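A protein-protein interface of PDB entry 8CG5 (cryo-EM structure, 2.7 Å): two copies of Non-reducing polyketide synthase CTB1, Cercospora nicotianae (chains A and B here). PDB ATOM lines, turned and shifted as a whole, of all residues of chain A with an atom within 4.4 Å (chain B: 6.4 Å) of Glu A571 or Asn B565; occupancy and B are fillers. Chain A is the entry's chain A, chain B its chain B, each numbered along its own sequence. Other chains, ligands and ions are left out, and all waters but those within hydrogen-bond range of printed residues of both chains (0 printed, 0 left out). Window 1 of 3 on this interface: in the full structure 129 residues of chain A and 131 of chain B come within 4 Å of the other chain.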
ATOM      1  N   ARG A 498      18.963   4.981   9.312  1.00  0.00           N
ATOM      2  CA  ARG A 498      20.307   5.545   9.325  1.00  0.00           C
ATOM      3  C   ARG A 498      21.318   4.651   8.618  1.00  0.00           C
ATOM      4  O   ARG A 498      22.524   4.810   8.823  1.00  0.00           O
ATOM      5  CB  ARG A 498      20.759   5.804  10.762  1.00  0.00           C
ATOM      6  CG  ARG A 498      19.727   6.500  11.630  1.00  0.00           C
ATOM      7  CD  ARG A 498      19.509   7.931  11.187  1.00  0.00           C
ATOM      8  NE  ARG A 498      20.701   8.746  11.384  1.00  0.00           N
ATOM      9  CZ  ARG A 498      21.060   9.761  10.610  1.00  0.00           C
ATOM     10  NH1 ARG A 498      20.326  10.138   9.576  1.00  0.00           N
ATOM     11  NH2 ARG A 498      22.182  10.417  10.881  1.00  0.00           N
ATOM     12  N   PRO A 545      19.730   5.991   2.007  1.00  0.00           N
ATOM     13  CA  PRO A 545      20.040   6.099   0.578  1.00  0.00           C
ATOM     14  C   PRO A 545      20.717   4.845   0.047  1.00  0.00           C
ATOM     15  O   PRO A 545      21.493   4.188   0.741  1.00  0.00           O
ATOM     16  CB  PRO A 545      20.976   7.311   0.506  1.00  0.00           C
ATOM     17  CG  PRO A 545      21.477   7.511   1.890  1.00  0.00           C
ATOM     18  CD  PRO A 545      20.410   7.022   2.805  1.00  0.00           C
ATOM     19  N   ALA A 566      28.825  10.517   2.512  1.00  0.00           N
ATOM     20  CA  ALA A 566      27.532  10.466   3.186  1.00  0.00           C
ATOM     21  C   ALA A 566      27.703  10.377   4.696  1.00  0.00           C
ATOM     22  O   ALA A 566      26.959  11.011   5.450  1.00  0.00           O
ATOM     23  CB  ALA A 566      26.717   9.282   2.671  1.00  0.00           C
ATOM     24  N   ARG A 569      28.839  13.788   6.197  1.00  0.00           N
ATOM     25  CA  ARG A 569      27.802  14.806   6.222  1.00  0.00           C
ATOM     26  C   ARG A 569      26.711  14.514   7.239  1.00  0.00           C
ATOM     27  O   ARG A 569      25.817  15.347   7.422  1.00  0.00           O
ATOM     28  CB  ARG A 569      27.170  14.954   4.837  1.00  0.00           C
ATOM     29  CG  ARG A 569      28.045  15.693   3.836  1.00  0.00           C
ATOM     30  CD  ARG A 569      27.395  16.980   3.364  1.00  0.00           C
ATOM     31  NE  ARG A 569      26.047  16.746   2.861  1.00  0.00           N
ATOM     32  CZ  ARG A 569      24.998  17.521   3.106  1.00  0.00           C
ATOM     33  NH1 ARG A 569      25.104  18.626   3.827  1.00  0.00           N
ATOM     34  NH2 ARG A 569      23.811  17.177   2.615  1.00  0.00           N
ATOM     35  N   GLY A 570      26.757  13.363   7.900  1.00  0.00           N
ATOM     36  CA  GLY A 570      25.781  13.036   8.915  1.00  0.00           C
ATOM     37  C   GLY A 570      24.449  12.557   8.394  1.00  0.00           C
ATOM     38  O   GLY A 570      23.494  12.478   9.172  1.00  0.00           O
ATOM     39  N   GLU A 571      24.347  12.238   7.107  1.00  0.00           N
ATOM     40  CA  GLU A 571      23.093  11.769   6.541  1.00  0.00           C
ATOM     41  C   GLU A 571      22.889  10.270   6.714  1.00  0.00           C
ATOM     42  O   GLU A 571      21.802   9.771   6.406  1.00  0.00           O
ATOM     43  CB  GLU A 571      23.018  12.148   5.059  1.00  0.00           C
ATOM     44  CG  GLU A 571      23.418  11.060   4.088  1.00  0.00           C
ATOM     45  CD  GLU A 571      23.428  11.553   2.658  1.00  0.00           C
ATOM     46  OE1 GLU A 571      23.719  12.749   2.448  1.00  0.00           O
ATOM     47  OE2 GLU A 571      23.146  10.750   1.745  1.00  0.00           O
ATOM     48  N   VAL A 572      23.900   9.544   7.191  1.00  0.00           N
ATOM     49  CA  VAL A 572      23.749   8.149   7.585  1.00  0.00           C
ATOM     50  C   VAL A 572      24.661   7.895   8.774  1.00  0.00           C
ATOM     51  O   VAL A 572      25.586   8.662   9.048  1.00  0.00           O
ATOM     52  CB  VAL A 572      24.073   7.160   6.441  1.00  0.00           C
ATOM     53  CG1 VAL A 572      23.095   7.329   5.298  1.00  0.00           C
ATOM     54  CG2 VAL A 572      25.499   7.346   5.959  1.00  0.00           C
ATOM     55  N   ILE B 384      22.747  26.319  -3.813  1.00  0.00           N
ATOM     56  CA  ILE B 384      23.455  25.902  -5.017  1.00  0.00           C
ATOM     57  C   ILE B 384      22.720  26.471  -6.221  1.00  0.00           C
ATOM     58  O   ILE B 384      21.516  26.244  -6.385  1.00  0.00           O
ATOM     59  CB  ILE B 384      23.558  24.370  -5.107  1.00  0.00           C
ATOM     60  CG1 ILE B 384      24.635  23.863  -4.150  1.00  0.00           C
ATOM     61  CG2 ILE B 384      23.874  23.939  -6.524  1.00  0.00           C
ATOM     62  CD1 ILE B 384      24.479  22.413  -3.783  1.00  0.00           C
ATOM     63  N   LEU B 560      22.565  14.378  -9.184  1.00  0.00           N
ATOM     64  CA  LEU B 560      22.491  15.756  -8.710  1.00  0.00           C
ATOM     65  C   LEU B 560      22.750  15.830  -7.210  1.00  0.00           C
ATOM     66  O   LEU B 560      23.458  16.724  -6.736  1.00  0.00           O
ATOM     67  CB  LEU B 560      21.127  16.347  -9.056  1.00  0.00           C
ATOM     68  CG  LEU B 560      20.866  17.790  -8.631  1.00  0.00           C
ATOM     69  CD1 LEU B 560      21.920  18.723  -9.189  1.00  0.00           C
ATOM     70  CD2 LEU B 560      19.489  18.218  -9.088  1.00  0.00           C
ATOM     71  N   HIS B 561      22.185  14.894  -6.448  1.00  0.00           N
ATOM     72  CA  HIS B 561      22.431  14.853  -5.012  1.00  0.00           C
ATOM     73  C   HIS B 561      23.909  14.649  -4.715  1.00  0.00           C
ATOM     74  O   HIS B 561      24.472  15.314  -3.839  1.00  0.00           O
ATOM     75  CB  HIS B 561      21.603  13.739  -4.375  1.00  0.00           C
ATOM     76  CG  HIS B 561      21.685  13.702  -2.881  1.00  0.00           C
ATOM     77  ND1 HIS B 561      21.147  12.678  -2.133  1.00  0.00           N
ATOM     78  CD2 HIS B 561      22.242  14.560  -1.996  1.00  0.00           C
ATOM     79  CE1 HIS B 561      21.370  12.907  -0.852  1.00  0.00           C
ATOM     80  NE2 HIS B 561      22.033  14.044  -0.742  1.00  0.00           N
ATOM     81  N   MET B 562      24.550  13.725  -5.429  1.00  0.00           N
ATOM     82  CA  MET B 562      25.971  13.480  -5.204  1.00  0.00           C
ATOM     83  C   MET B 562      26.797  14.713  -5.546  1.00  0.00           C
ATOM     84  O   MET B 562      27.741  15.060  -4.825  1.00  0.00           O
ATOM     85  CB  MET B 562      26.430  12.282  -6.031  1.00  0.00           C
ATOM     86  CG  MET B 562      25.661  11.003  -5.744  1.00  0.00           C
ATOM     87  SD  MET B 562      26.519   9.900  -4.612  1.00  0.00           S
ATOM     88  CE  MET B 562      25.825  10.425  -3.048  1.00  0.00           C
ATOM     89  N   ALA B 563      26.456  15.391  -6.643  1.00  0.00           N
ATOM     90  CA  ALA B 563      27.176  16.600  -7.022  1.00  0.00           C
ATOM     91  C   ALA B 563      27.024  17.683  -5.965  1.00  0.00           C
ATOM     92  O   ALA B 563      27.995  18.365  -5.621  1.00  0.00           O
ATOM     93  CB  ALA B 563      26.677  17.104  -8.374  1.00  0.00           C
ATOM     94  N   CYS B 564      25.810  17.857  -5.440  1.00  0.00           N
ATOM     95  CA  CYS B 564      25.607  18.828  -4.371  1.00  0.00           C
ATOM     96  C   CYS B 564      26.411  18.453  -3.135  1.00  0.00           C
ATOM     97  O   CYS B 564      27.001  19.320  -2.482  1.00  0.00           O
ATOM     98  CB  CYS B 564      24.120  18.933  -4.037  1.00  0.00           C
ATOM     99  SG  CYS B 564      23.104  19.586  -5.378  1.00  0.00           S
ATOM    100  N   ASN B 565      26.452  17.162  -2.800  1.00  0.00           N
ATOM    101  CA  ASN B 565      27.272  16.717  -1.679  1.00  0.00           C
ATOM    102  C   ASN B 565      28.728  17.106  -1.888  1.00  0.00           C
ATOM    103  O   ASN B 565      29.388  17.604  -0.970  1.00  0.00           O
ATOM    104  CB  ASN B 565      27.146  15.204  -1.508  1.00  0.00           C
ATOM    105  CG  ASN B 565      26.041  14.816  -0.558  1.00  0.00           C
ATOM    106  OD1 ASN B 565      25.005  15.474  -0.491  1.00  0.00           O
ATOM    107  ND2 ASN B 565      26.250  13.735   0.183  1.00  0.00           N
ATOM    108  N   ALA B 566      29.248  16.882  -3.096  1.00  0.00           N
ATOM    109  CA  ALA B 566      30.618  17.288  -3.390  1.00  0.00           C
ATOM    110  C   ALA B 566      30.775  18.799  -3.299  1.00  0.00           C
ATOM    111  O   ALA B 566      31.782  19.298  -2.785  1.00  0.00           O
ATOM    112  CB  ALA B 566      31.027  16.793  -4.775  1.00  0.00           C
ATOM    113  N   LEU B 567      29.787  19.546  -3.795  1.00  0.00           N
ATOM    114  CA  LEU B 567      29.863  21.001  -3.744  1.00  0.00           C
ATOM    115  C   LEU B 567      29.810  21.520  -2.316  1.00  0.00           C
ATOM    116  O   LEU B 567      30.424  22.547  -2.008  1.00  0.00           O
ATOM    117  CB  LEU B 567      28.723  21.612  -4.556  1.00  0.00           C
ATOM    118  CG  LEU B 567      28.955  21.761  -6.058  1.00  0.00           C
ATOM    119  CD1 LEU B 567      27.629  21.829  -6.784  1.00  0.00           C
ATOM    120  CD2 LEU B 567      29.785  22.991  -6.352  1.00  0.00           C
ATOM    121  N   TRP B 568      29.084  20.835  -1.434  1.00  0.00           N
ATOM    122  CA  TRP B 568      28.861  21.330  -0.084  1.00  0.00           C
ATOM    123  C   TRP B 568      30.062  21.145   0.832  1.00  0.00           C
ATOM    124  O   TRP B 568      30.075  21.727   1.920  1.00  0.00           O
ATOM    125  CB  TRP B 568      27.646  20.635   0.536  1.00  0.00           C
ATOM    126  CG  TRP B 568      26.343  21.298   0.217  1.00  0.00           C
ATOM    127  CD1 TRP B 568      26.111  22.634   0.089  1.00  0.00           C
ATOM    128  CD2 TRP B 568      25.087  20.652  -0.011  1.00  0.00           C
ATOM    129  NE1 TRP B 568      24.793  22.860  -0.208  1.00  0.00           N
ATOM    130  CE2 TRP B 568      24.142  21.658  -0.274  1.00  0.00           C
ATOM    131  CE3 TRP B 568      24.672  19.319  -0.019  1.00  0.00           C
ATOM    132  CZ2 TRP B 568      22.809  21.374  -0.542  1.00  0.00           C
ATOM    133  CZ3 TRP B 568      23.349  19.040  -0.286  1.00  0.00           C
ATOM    134  CH2 TRP B 568      22.433  20.062  -0.543  1.00  0.00           C
ATOM    135  N   ARG B 569      31.063  20.360   0.434  1.00  0.00           N
ATOM    136  CA  ARG B 569      32.259  20.177   1.247  1.00  0.00           C
ATOM    137  C   ARG B 569      33.529  20.586   0.510  1.00  0.00           C
ATOM    138  O   ARG B 569      34.626  20.174   0.898  1.00  0.00           O
ATOM    139  CB  ARG B 569      32.367  18.733   1.733  1.00  0.00           C
ATOM    140  CG  ARG B 569      31.890  17.682   0.764  1.00  0.00           C
ATOM    141  CD  ARG B 569      32.755  16.455   0.906  1.00  0.00           C
ATOM    142  NE  ARG B 569      32.778  15.995   2.288  1.00  0.00           N
ATOM    143  CZ  ARG B 569      33.721  15.222   2.807  1.00  0.00           C
ATOM    144  NH1 ARG B 569      34.719  14.760   2.073  1.00  0.00           N
ATOM    145  NH2 ARG B 569      33.666  14.915   4.098  1.00  0.00           N
ATOM    146  N   GLY B 570      33.408  21.390  -0.541  1.00  0.00           N
ATOM    147  CA  GLY B 570      34.566  21.994  -1.163  1.00  0.00           C
ATOM    148  C   GLY B 570      35.385  21.085  -2.047  1.00  0.00           C
ATOM    149  O   GLY B 570      36.473  21.486  -2.473  1.00  0.00           O
ATOM    150  N   GLU B 571      34.909  19.875  -2.340  1.00  0.00           N
ATOM    151  CA  GLU B 571      35.656  18.999  -3.237  1.00  0.00           C
ATOM    152  C   GLU B 571      35.797  19.629  -4.613  1.00  0.00           C
ATOM    153  O   GLU B 571      36.868  19.567  -5.229  1.00  0.00           O
ATOM    154  CB  GLU B 571      34.971  17.639  -3.341  1.00  0.00           C
ATOM    155  CG  GLU B 571      34.502  17.076  -2.017  1.00  0.00           C
ATOM    156  CD  GLU B 571      34.745  15.588  -1.901  1.00  0.00           C
ATOM    157  OE1 GLU B 571      33.949  14.812  -2.468  1.00  0.00           O
ATOM    158  OE2 GLU B 571      35.728  15.194  -1.240  1.00  0.00           O
ATOM    159  N   ILE B 645      18.235  18.784  -0.723  1.00  0.00           N
ATOM    160  CA  ILE B 645      17.985  17.542  -1.445  1.00  0.00           C
ATOM    161  C   ILE B 645      18.234  16.387  -0.489  1.00  0.00           C
ATOM    162  O   ILE B 645      19.146  16.439   0.340  1.00  0.00           O
ATOM    163  CB  ILE B 645      18.867  17.439  -2.707  1.00  0.00           C
ATOM    164  CG1 ILE B 645      18.626  16.111  -3.424  1.00  0.00           C
ATOM    165  CG2 ILE B 645      20.335  17.591  -2.352  1.00  0.00           C
ATOM    166  CD1 ILE B 645      18.737  16.207  -4.923  1.00  0.00           C
ATOM    167  N   THR B 647      17.520  11.806   0.096  1.00  0.00           N
ATOM    168  CA  THR B 647      17.215  10.509  -0.489  1.00  0.00           C
ATOM    169  C   THR B 647      16.871   9.527   0.621  1.00  0.00           C
ATOM    170  O   THR B 647      17.359   9.643   1.747  1.00  0.00           O
ATOM    171  CB  THR B 647      18.397   9.972  -1.307  1.00  0.00           C
ATOM    172  OG1 THR B 647      18.876  10.994  -2.188  1.00  0.00           O
ATOM    173  CG2 THR B 647      17.985   8.763  -2.127  1.00  0.00           C
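A ring nitrogen (ND1) of His B561 sits at hydrogen-bond distance from the side-chain hydroxyl (OG1) of Thr B647.
O of Ala A566 sits at hydrogen-bond distance from N of Glu A571, at 3.3 Å.
NE2 of His B561 sits close to OD1 of Asn B565 (3.3 Å).
Among the printed residues, pairs that only touch across the chains: Arg A569 with Asn B565, Arg A569 with Trp B568, Glu A571 with His B561 and Glu A571 with Asn B565.
Of the printed residues of chain B, Arg A569 touches Asn B565 (3.7 Å) and Trp B568 (3.5 Å).
Printed residues of chain A within 4 Å of His B561: Glu A571.
Cys B564 touches none of the printed residues of chain A.
Asn B565 touches two residues of chain A.
The nearest printed residue of chain A that does not touch His B561 is Arg A569 (4.9 Å).
Of the 15 printed residues of chain B, 3 touch a printed residue of chain A.
Hydrophobic or aromatic side chains of chain B within 4 Å of the printed part of chain A: His B561 and Trp B568.
Of the 7 printed residues of chain A, 2 touch a printed residue of chain B.
Among the printed residues, no Asp or Glu carboxylate lies within 4 Å of a Lys or Arg side-chain nitrogen of the other chain.
Positions printed for both chains: 566, 569, 570 and 571.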
